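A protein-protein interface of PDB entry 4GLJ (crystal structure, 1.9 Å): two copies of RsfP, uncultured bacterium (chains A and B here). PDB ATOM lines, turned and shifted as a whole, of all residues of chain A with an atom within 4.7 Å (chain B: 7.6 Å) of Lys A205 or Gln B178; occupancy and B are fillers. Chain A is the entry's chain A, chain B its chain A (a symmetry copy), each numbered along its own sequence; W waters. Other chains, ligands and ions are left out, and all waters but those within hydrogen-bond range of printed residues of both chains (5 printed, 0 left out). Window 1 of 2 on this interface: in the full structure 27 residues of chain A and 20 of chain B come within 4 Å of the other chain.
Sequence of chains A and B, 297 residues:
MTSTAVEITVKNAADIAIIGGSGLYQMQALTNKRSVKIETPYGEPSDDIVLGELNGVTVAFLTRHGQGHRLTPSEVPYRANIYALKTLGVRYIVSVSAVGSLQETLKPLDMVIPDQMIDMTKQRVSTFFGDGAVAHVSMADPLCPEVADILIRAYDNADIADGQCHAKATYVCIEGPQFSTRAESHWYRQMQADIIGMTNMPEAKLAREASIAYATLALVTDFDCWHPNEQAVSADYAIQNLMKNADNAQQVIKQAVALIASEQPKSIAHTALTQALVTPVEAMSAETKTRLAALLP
N of Asp A119 sits at hydrogen-bond distance from OE2 of Glu B184 (2.8 Å).
The side-chain carboxylate (OD1) of Asp A119 lies within salt-bridge range of the side-chain amino group (NZ) of Lys B122 (3.6 Å).
The side-chain carboxylate (OE2) of Glu A209 is in hydrogen-bond range of the side-chain amide nitrogen (NE2) of Gln B178, 2.8 Å away.
The backbone carbonyl oxygen of Phe B179 sits close to the backbone NH of Met A139 (3.5 Å).
O of Val A137 lies within hydrogen-bond range of N of Phe B179 (3.0 Å).
The backbone carbonyl oxygen of Ser A126 lies within hydrogen-bond range of the side-chain amide nitrogen of Gln B178 (2.8 Å).
The backbone NH (N) of Lys B122 lies within hydrogen-bond range of the side-chain carboxylate (OE1) of Glu B175, 2.8 Å away.
OD2 of Asp A119 is in salt-bridge range of NZ of Lys A205 (2.7 Å).
The side-chain hydroxyl (OG1) of Thr A127 sits at hydrogen-bond distance from the side-chain carboxylate (OE2) of Glu A209.
OG1 of Thr B181 is in hydrogen-bond range of N of Glu B184 (3.0 Å).
Among the printed residues, pairs that only touch across the chains: Thr A127 with Pro B177 (3.4 Å), Thr A127 with Gln B178 (3.7 Å), Val A137 with Gln B178 (3.4 Å), Met A139 with Gln B178 (3.5 Å), Met A139 with Ser B180 (3.8 Å), Met A139 with Thr B181 (3.2 Å) and Lys A205 with Gln B178 (3.3 Å).
Glu A203 touches none of the printed residues of chain B.
No residue of chain B comes within 4 Å of Ala A204.
Lys A205 touches just one residue of chain B: Gln B178.
Leu A206 touches none of the printed residues of chain B.
Printed residues of chain B within 4 Å of Glu A209: Gln B178.
Of the printed residues of chain A, Lys B122 touches Asp A119.
Of the printed residues of chain A, Pro B177 touches Thr A127 (3.4 Å).
Gln B178 touches just these residues of chain A: Ser A126 (2.8 Å), Thr A127 (3.7 Å), Val A137 (3.4 Å), Met A139 (3.5 Å), Lys A205 (3.3 Å) and Glu A209 (2.8 Å).
Printed residues of chain A within 4 Å of Phe B179: Val A137 (3.0 Å) and Met A139 (3.3 Å).
The nearest residue of chain B that does not touch Lys A205 is Lys B122 (4.8 Å).
The nearest printed residue of chain B that does not touch Glu A209 is Pro B177 (4.1 Å).
Hydrophobic or aromatic side chains of chain A that line the printed part of chain B: Val A137 and Met A139.
Printed residues of chain B that touch a printed residue of chain A: Lys B122, Pro B177, Gln B178, Phe B179, Ser B180, Thr B181 and Glu B184.
Hydrophobic or aromatic side chains of chain B within 4 Å of the printed part of chain A: Pro B177 and Phe B179.
Along chain B the printed residues that touch a printed residue of chain A span positions 122 to 184.
No position is printed for both chains.
Of the 13 pairs that touch across the chains among the printed residues, none has its exchanged pair printed and touching as well.
Water W1 lies within hydrogen-bond range of NZ of Lys A205 (2.6 Å) and OE2 of Glu B184 (3.0 Å).
Water W3 lies within hydrogen-bond range of the side-chain amide oxygen of Gln B178, the backbone carbonyl oxygen of Gly B176, the side-chain hydroxyl of Ser A126 and the side-chain amino group of Lys A205.
Water W4 bridges the backbone NH of Met A139 (2.8 Å) and the backbone carbonyl oxygen of Ser B180 (3.0 Å).
Water W5 lies within hydrogen-bond range of O of Gln B178 and NZ of Lys A205.
Water W2 bridges NZ of Lys B122 (2.9 Å) and NZ of Lys A205 (3.1 Å).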
ATOM      1  N   ASP A 119     -26.511  -6.466  15.921  1.00  0.00           N
ATOM      2  CA  ASP A 119     -27.768  -6.066  15.334  1.00  0.00           C
ATOM      3  C   ASP A 119     -27.539  -5.215  14.101  1.00  0.00           C
ATOM      4  O   ASP A 119     -27.232  -4.031  14.210  1.00  0.00           O
ATOM      5  CB  ASP A 119     -28.611  -5.298  16.334  1.00  0.00           C
ATOM      6  CG  ASP A 119     -30.017  -5.015  15.815  1.00  0.00           C
ATOM      7  OD1 ASP A 119     -30.361  -5.438  14.694  1.00  0.00           O
ATOM      8  OD2 ASP A 119     -30.789  -4.364  16.568  1.00  0.00           O
ATOM      9  N   SER A 126     -37.077  -1.230  18.041  1.00  0.00           N
ATOM     10  CA  SER A 126     -36.209  -2.151  18.792  1.00  0.00           C
ATOM     11  C   SER A 126     -36.184  -1.836  20.320  1.00  0.00           C
ATOM     12  O   SER A 126     -35.302  -2.295  21.052  1.00  0.00           O
ATOM     13  CB  SER A 126     -34.784  -2.125  18.194  1.00  0.00           C
ATOM     14  OG  SER A 126     -34.362  -0.749  18.202  1.00  0.00           O
ATOM     15  N   THR A 127     -37.218  -1.140  20.782  1.00  0.00           N
ATOM     16  CA  THR A 127     -37.375  -0.813  22.209  1.00  0.00           C
ATOM     17  C   THR A 127     -38.841  -0.583  22.490  1.00  0.00           C
ATOM     18  O   THR A 127     -39.654  -0.245  21.607  1.00  0.00           O
ATOM     19  CB  THR A 127     -36.563   0.464  22.580  1.00  0.00           C
ATOM     20  OG1 THR A 127     -36.710   0.759  23.974  1.00  0.00           O
ATOM     21  CG2 THR A 127     -37.041   1.692  21.797  1.00  0.00           C
ATOM     22  N   VAL A 137     -31.153  -0.339  28.809  1.00  0.00           N
ATOM     23  CA  VAL A 137     -30.653  -1.639  29.373  1.00  0.00           C
ATOM     24  C   VAL A 137     -29.289  -1.979  28.746  1.00  0.00           C
ATOM     25  O   VAL A 137     -28.982  -1.576  27.626  1.00  0.00           O
ATOM     26  CB  VAL A 137     -31.659  -2.788  29.179  1.00  0.00           C
ATOM     27  CG1 VAL A 137     -32.957  -2.452  29.895  1.00  0.00           C
ATOM     28  CG2 VAL A 137     -31.946  -3.053  27.692  1.00  0.00           C
ATOM     29  N   MET A 139     -26.917  -4.529  26.888  1.00  0.00           N
ATOM     30  CA  MET A 139     -27.006  -5.751  26.102  1.00  0.00           C
ATOM     31  C   MET A 139     -25.607  -6.344  25.986  1.00  0.00           C
ATOM     32  O   MET A 139     -25.379  -7.148  25.088  1.00  0.00           O
ATOM     33  CB  MET A 139     -27.504  -5.414  24.711  1.00  0.00           C
ATOM     34  CG  MET A 139     -28.973  -4.981  24.695  1.00  0.00           C
ATOM     35  SD  MET A 139     -30.086  -6.237  25.317  1.00  0.00           S
ATOM     36  CE  MET A 139     -29.947  -7.663  24.185  1.00  0.00           C
ATOM     37  N   MET A 201     -32.883 -10.215  16.549  1.00  0.00           N
ATOM     38  CA  MET A 201     -32.985  -8.781  16.886  1.00  0.00           C
ATOM     39  C   MET A 201     -34.189  -8.231  16.149  1.00  0.00           C
ATOM     40  O   MET A 201     -34.318  -8.456  14.956  1.00  0.00           O
ATOM     41  CB  MET A 201     -31.705  -8.028  16.489  1.00  0.00           C
ATOM     42  CG  MET A 201     -30.489  -8.369  17.355  1.00  0.00           C
ATOM     43  SD  MET A 201     -30.698  -7.543  18.972  1.00  0.00           S
ATOM     44  CE  MET A 201     -29.163  -7.981  19.781  1.00  0.00           C
ATOM     45  N   PRO A 202     -35.080  -7.491  16.822  1.00  0.00           N
ATOM     46  CA  PRO A 202     -34.865  -6.887  18.160  1.00  0.00           C
ATOM     47  C   PRO A 202     -35.370  -7.782  19.301  1.00  0.00           C
ATOM     48  O   PRO A 202     -35.356  -7.330  20.424  1.00  0.00           O
ATOM     49  CB  PRO A 202     -35.711  -5.603  18.083  1.00  0.00           C
ATOM     50  CG  PRO A 202     -36.884  -6.062  17.247  1.00  0.00           C
ATOM     51  CD  PRO A 202     -36.244  -6.873  16.137  1.00  0.00           C
ATOM     52  N   GLU A 203     -35.735  -9.032  18.989  1.00  0.00           N
ATOM     53  CA  GLU A 203     -36.343  -9.963  20.009  1.00  0.00           C
ATOM     54  C   GLU A 203     -35.471 -10.042  21.260  1.00  0.00           C
ATOM     55  O   GLU A 203     -36.018  -9.910  22.378  1.00  0.00           O
ATOM     56  CB  GLU A 203     -36.514 -11.332  19.395  1.00  0.00           C
ATOM     57  CG  GLU A 203     -37.663 -12.162  19.881  1.00  0.00           C
ATOM     58  CD  GLU A 203     -37.782 -13.444  19.069  1.00  0.00           C
ATOM     59  OE1 GLU A 203     -36.909 -14.348  19.278  1.00  0.00           O
ATOM     60  OE2 GLU A 203     -38.660 -13.542  18.161  1.00  0.00           O
ATOM     61  N   ALA A 204     -34.135 -10.149  21.095  1.00  0.00           N
ATOM     62  CA  ALA A 204     -33.255 -10.235  22.294  1.00  0.00           C
ATOM     63  C   ALA A 204     -33.261  -8.930  23.133  1.00  0.00           C
ATOM     64  O   ALA A 204     -33.190  -8.979  24.386  1.00  0.00           O
ATOM     65  CB  ALA A 204     -31.802 -10.625  21.951  1.00  0.00           C
ATOM     66  N   LYS A 205     -33.258  -7.771  22.447  1.00  0.00           N
ATOM     67  CA  LYS A 205     -33.313  -6.457  23.124  1.00  0.00           C
ATOM     68  C   LYS A 205     -34.647  -6.323  23.933  1.00  0.00           C
ATOM     69  O   LYS A 205     -34.666  -5.810  25.057  1.00  0.00           O
ATOM     70  CB  LYS A 205     -33.225  -5.322  22.047  1.00  0.00           C
ATOM     71  CG  LYS A 205     -31.797  -5.202  21.470  1.00  0.00           C
ATOM     72  CD  LYS A 205     -31.777  -4.111  20.379  1.00  0.00           C
ATOM     73  CE  LYS A 205     -30.278  -3.869  20.076  1.00  0.00           C
ATOM     74  NZ  LYS A 205     -30.056  -3.028  18.826  1.00  0.00           N
ATOM     75  N   LEU A 206     -35.738  -6.610  23.286  1.00  0.00           N
ATOM     76  CA  LEU A 206     -37.065  -6.489  23.878  1.00  0.00           C
ATOM     77  C   LEU A 206     -37.225  -7.436  25.088  1.00  0.00           C
ATOM     78  O   LEU A 206     -37.776  -7.043  26.120  1.00  0.00           O
ATOM     79  CB  LEU A 206     -38.154  -6.745  22.807  1.00  0.00           C
ATOM     80  CG  LEU A 206     -38.097  -5.626  21.706  1.00  0.00           C
ATOM     81  CD1 LEU A 206     -38.911  -6.019  20.461  1.00  0.00           C
ATOM     82  CD2 LEU A 206     -38.591  -4.264  22.248  1.00  0.00           C
ATOM     83  N   ALA A 207     -36.733  -8.657  24.957  1.00  0.00           N
ATOM     84  CA  ALA A 207     -36.783  -9.647  26.056  1.00  0.00           C
ATOM     85  C   ALA A 207     -35.983  -9.063  27.226  1.00  0.00           C
ATOM     86  O   ALA A 207     -36.415  -9.150  28.404  1.00  0.00           O
ATOM     87  CB  ALA A 207     -36.167 -10.993  25.584  1.00  0.00           C
ATOM     88  N   ARG A 208     -34.819  -8.452  26.948  1.00  0.00           N
ATOM     89  CA  ARG A 208     -34.014  -7.874  28.030  1.00  0.00           C
ATOM     90  C   ARG A 208     -34.773  -6.725  28.720  1.00  0.00           C
ATOM     91  O   ARG A 208     -34.807  -6.633  29.958  1.00  0.00           O
ATOM     92  CB  ARG A 208     -32.670  -7.380  27.489  1.00  0.00           C
ATOM     93  CG  ARG A 208     -31.680  -6.885  28.536  1.00  0.00           C
ATOM     94  CD  ARG A 208     -31.308  -7.867  29.678  1.00  0.00           C
ATOM     95  NE  ARG A 208     -30.857  -9.155  29.118  1.00  0.00           N
ATOM     96  CZ  ARG A 208     -29.582  -9.418  28.813  1.00  0.00           C
ATOM     97  NH1 ARG A 208     -28.627  -8.489  29.063  1.00  0.00           N
ATOM     98  NH2 ARG A 208     -29.220 -10.628  28.376  1.00  0.00           N
ATOM     99  N   GLU A 209     -35.391  -5.845  27.922  1.00  0.00           N
ATOM    100  CA  GLU A 209     -36.173  -4.738  28.501  1.00  0.00           C
ATOM    101  C   GLU A 209     -37.351  -5.238  29.308  1.00  0.00           C
ATOM    102  O   GLU A 209     -37.833  -4.522  30.225  1.00  0.00           O
ATOM    103  CB  GLU A 209     -36.729  -3.814  27.412  1.00  0.00           C
ATOM    104  CG  GLU A 209     -35.616  -3.001  26.739  1.00  0.00           C
ATOM    105  CD  GLU A 209     -36.153  -2.002  25.741  1.00  0.00           C
ATOM    106  OE1 GLU A 209     -37.356  -2.146  25.352  1.00  0.00           O
ATOM    107  OE2 GLU A 209     -35.360  -1.085  25.326  1.00  0.00           O
ATOM    108  N   LYS B 122     -30.059   4.410  12.526  1.00  0.00           N
ATOM    109  CA  LYS B 122     -30.896   3.648  11.585  1.00  0.00           C
ATOM    110  C   LYS B 122     -32.155   4.355  11.205  1.00  0.00           C
ATOM    111  O   LYS B 122     -32.600   4.333  10.022  1.00  0.00           O
ATOM    112  CB  LYS B 122     -31.226   2.304  12.244  1.00  0.00           C
ATOM    113  CG  LYS B 122     -29.972   1.420  12.475  1.00  0.00           C
ATOM    114  CD  LYS B 122     -30.348   0.231  13.357  1.00  0.00           C
ATOM    115  CE  LYS B 122     -29.102  -0.646  13.691  1.00  0.00           C
ATOM    116  NZ  LYS B 122     -29.473  -1.997  14.179  1.00  0.00           N
ATOM    117  N   ILE B 174     -24.616   5.320  17.526  1.00  0.00           N
ATOM    118  CA  ILE B 174     -25.510   4.183  17.322  1.00  0.00           C
ATOM    119  C   ILE B 174     -26.919   4.638  17.623  1.00  0.00           C
ATOM    120  O   ILE B 174     -27.161   5.742  18.217  1.00  0.00           O
ATOM    121  CB  ILE B 174     -25.095   2.977  18.221  1.00  0.00           C
ATOM    122  CG1 ILE B 174     -25.253   3.323  19.731  1.00  0.00           C
ATOM    123  CG2 ILE B 174     -23.676   2.453  17.838  1.00  0.00           C
ATOM    124  CD1 ILE B 174     -25.261   2.059  20.624  1.00  0.00           C
ATOM    125  N   GLU B 175     -27.868   3.814  17.205  1.00  0.00           N
ATOM    126  CA  GLU B 175     -29.281   4.148  17.324  1.00  0.00           C
ATOM    127  C   GLU B 175     -29.729   4.160  18.804  1.00  0.00           C
ATOM    128  O   GLU B 175     -30.446   5.053  19.181  1.00  0.00           O
ATOM    129  CB  GLU B 175     -30.131   3.123  16.515  1.00  0.00           C
ATOM    130  CG  GLU B 175     -31.630   3.437  16.496  1.00  0.00           C
ATOM    131  CD  GLU B 175     -31.873   4.871  15.965  1.00  0.00           C
ATOM    132  OE1 GLU B 175     -31.407   5.158  14.848  1.00  0.00           O
ATOM    133  OE2 GLU B 175     -32.533   5.760  16.626  1.00  0.00           O
ATOM    134  N   GLY B 176     -29.322   3.163  19.591  1.00  0.00           N
ATOM    135  CA  GLY B 176     -29.762   3.104  21.001  1.00  0.00           C
ATOM    136  C   GLY B 176     -31.168   2.496  20.975  1.00  0.00           C
ATOM    137  O   GLY B 176     -31.622   2.035  19.917  1.00  0.00           O
ATOM    138  N   PRO B 177     -31.897   2.510  22.109  1.00  0.00           N
ATOM    139  CA  PRO B 177     -31.405   3.044  23.359  1.00  0.00           C
ATOM    140  C   PRO B 177     -30.511   2.067  24.140  1.00  0.00           C
ATOM    141  O   PRO B 177     -29.918   2.512  25.119  1.00  0.00           O
ATOM    142  CB  PRO B 177     -32.719   3.365  24.112  1.00  0.00           C
ATOM    143  CG  PRO B 177     -33.670   2.243  23.673  1.00  0.00           C
ATOM    144  CD  PRO B 177     -33.313   2.069  22.200  1.00  0.00           C
ATOM    145  N   GLN B 178     -30.420   0.782  23.748  1.00  0.00           N
ATOM    146  CA  GLN B 178     -29.674  -0.168  24.610  1.00  0.00           C
ATOM    147  C   GLN B 178     -28.220   0.035  24.440  1.00  0.00           C
ATOM    148  O   GLN B 178     -27.805   0.469  23.365  1.00  0.00           O
ATOM    149  CB  GLN B 178     -30.066  -1.638  24.295  1.00  0.00           C
ATOM    150  CG  GLN B 178     -31.582  -1.864  24.476  1.00  0.00           C
ATOM    151  CD  GLN B 178     -32.339  -1.607  23.162  1.00  0.00           C
ATOM    152  OE1 GLN B 178     -31.710  -1.320  22.111  1.00  0.00           O
ATOM    153  NE2 GLN B 178     -33.645  -1.698  23.198  1.00  0.00           N
ATOM    154  N   PHE B 179     -27.424  -0.256  25.467  1.00  0.00           N
ATOM    155  CA  PHE B 179     -25.972  -0.230  25.255  1.00  0.00           C
ATOM    156  C   PHE B 179     -25.537  -1.427  24.430  1.00  0.00           C
ATOM    157  O   PHE B 179     -26.303  -2.366  24.247  1.00  0.00           O
ATOM    158  CB  PHE B 179     -25.212  -0.125  26.590  1.00  0.00           C
ATOM    159  CG  PHE B 179     -25.552   1.127  27.382  1.00  0.00           C
ATOM    160  CD1 PHE B 179     -25.248   2.398  26.865  1.00  0.00           C
ATOM    161  CD2 PHE B 179     -26.215   1.044  28.619  1.00  0.00           C
ATOM    162  CE1 PHE B 179     -25.558   3.557  27.601  1.00  0.00           C
ATOM    163  CE2 PHE B 179     -26.522   2.202  29.356  1.00  0.00           C
ATOM    164  CZ  PHE B 179     -26.174   3.452  28.863  1.00  0.00           C
ATOM    165  N   SER B 180     -24.364  -1.336  23.843  1.00  0.00           N
ATOM    166  CA  SER B 180     -23.867  -2.242  22.801  1.00  0.00           C
ATOM    167  C   SER B 180     -23.616  -3.603  23.353  1.00  0.00           C
ATOM    168  O   SER B 180     -23.201  -3.743  24.549  1.00  0.00           O
ATOM    169  CB  SER B 180     -22.519  -1.707  22.289  1.00  0.00           C
ATOM    170  OG  SER B 180     -22.766  -0.494  21.588  1.00  0.00           O
ATOM    171  N   THR B 181     -23.780  -4.625  22.511  1.00  0.00           N
ATOM    172  CA  THR B 181     -23.310  -5.960  22.916  1.00  0.00           C
ATOM    173  C   THR B 181     -21.758  -5.953  22.905  1.00  0.00           C
ATOM    174  O   THR B 181     -21.176  -5.062  22.279  1.00  0.00           O
ATOM    175  CB  THR B 181     -23.801  -7.071  21.925  1.00  0.00           C
ATOM    176  OG1 THR B 181     -23.069  -6.916  20.693  1.00  0.00           O
ATOM    177  CG2 THR B 181     -25.334  -6.997  21.636  1.00  0.00           C
ATOM    178  N   GLU B 184     -20.543  -6.094  19.349  1.00  0.00           N
ATOM    179  CA  GLU B 184     -20.646  -4.809  18.667  1.00  0.00           C
ATOM    180  C   GLU B 184     -19.513  -3.901  19.106  1.00  0.00           C
ATOM    181  O   GLU B 184     -18.871  -3.299  18.228  1.00  0.00           O
ATOM    182  CB  GLU B 184     -21.992  -4.103  18.919  1.00  0.00           C
ATOM    183  CG  GLU B 184     -23.163  -4.778  18.171  1.00  0.00           C
ATOM    184  CD  GLU B 184     -24.560  -4.480  18.757  1.00  0.00           C
ATOM    185  OE1 GLU B 184     -24.730  -3.738  19.828  1.00  0.00           O
ATOM    186  OE2 GLU B 184     -25.544  -4.946  18.088  1.00  0.00           O
ATOM    187  N   ILE B 196     -18.201   6.099  21.765  1.00  0.00           N
ATOM    188  CA  ILE B 196     -19.507   5.732  21.345  1.00  0.00           C
ATOM    189  C   ILE B 196     -20.564   6.583  21.993  1.00  0.00           C
ATOM    190  O   ILE B 196     -20.630   6.734  23.250  1.00  0.00           O
ATOM    191  CB  ILE B 196     -19.763   4.203  21.556  1.00  0.00           C
ATOM    192  CG1 ILE B 196     -21.218   3.814  21.128  1.00  0.00           C
ATOM    193  CG2 ILE B 196     -19.487   3.769  22.995  1.00  0.00           C
ATOM    194  CD1 ILE B 196     -21.244   2.378  20.655  1.00  0.00           C
ATOM    195  N   MET B 198     -24.955   8.278  21.212  1.00  0.00           N
ATOM    196  CA  MET B 198     -26.237   7.962  20.523  1.00  0.00           C
ATOM    197  C   MET B 198     -26.844   9.181  19.880  1.00  0.00           C
ATOM    198  O   MET B 198     -27.958   9.086  19.311  1.00  0.00           O
ATOM    199  CB  MET B 198     -27.219   7.346  21.535  1.00  0.00           C
ATOM    200  CG  MET B 198     -26.677   6.054  22.185  1.00  0.00           C
ATOM    201  SD  MET B 198     -27.921   5.319  23.255  1.00  0.00           S
ATOM    202  CE  MET B 198     -26.997   3.921  23.839  1.00  0.00           C
ATOM    203  N   ASP B 224     -17.315   1.361  27.474  1.00  0.00           N
ATOM    204  CA  ASP B 224     -18.466   0.710  26.938  1.00  0.00           C
ATOM    205  C   ASP B 224     -18.316  -0.614  27.674  1.00  0.00           C
ATOM    206  O   ASP B 224     -17.393  -0.792  28.478  1.00  0.00           O
ATOM    207  CB  ASP B 224     -18.426   0.690  25.418  1.00  0.00           C
ATOM    208  CG  ASP B 224     -19.783   0.471  24.835  1.00  0.00           C
ATOM    209  OD1 ASP B 224     -20.835   0.770  25.455  1.00  0.00           O
ATOM    210  OD2 ASP B 224     -19.841  -0.150  23.769  1.00  0.00           O
HETATM  211  O   HOH W   1     -27.489  -2.683  18.413  1.00  0.00           O
HETATM  212  O   HOH W   2     -30.304  -0.846  16.690  1.00  0.00           O
HETATM  213  O   HOH W   3     -31.869  -0.666  19.520  1.00  0.00           O
HETATM  214  O   HOH W   4     -24.469  -3.310  27.203  1.00  0.00           O
HETATM  215  O   HOH W   5     -28.444  -0.884  20.956  1.00  0.00           O
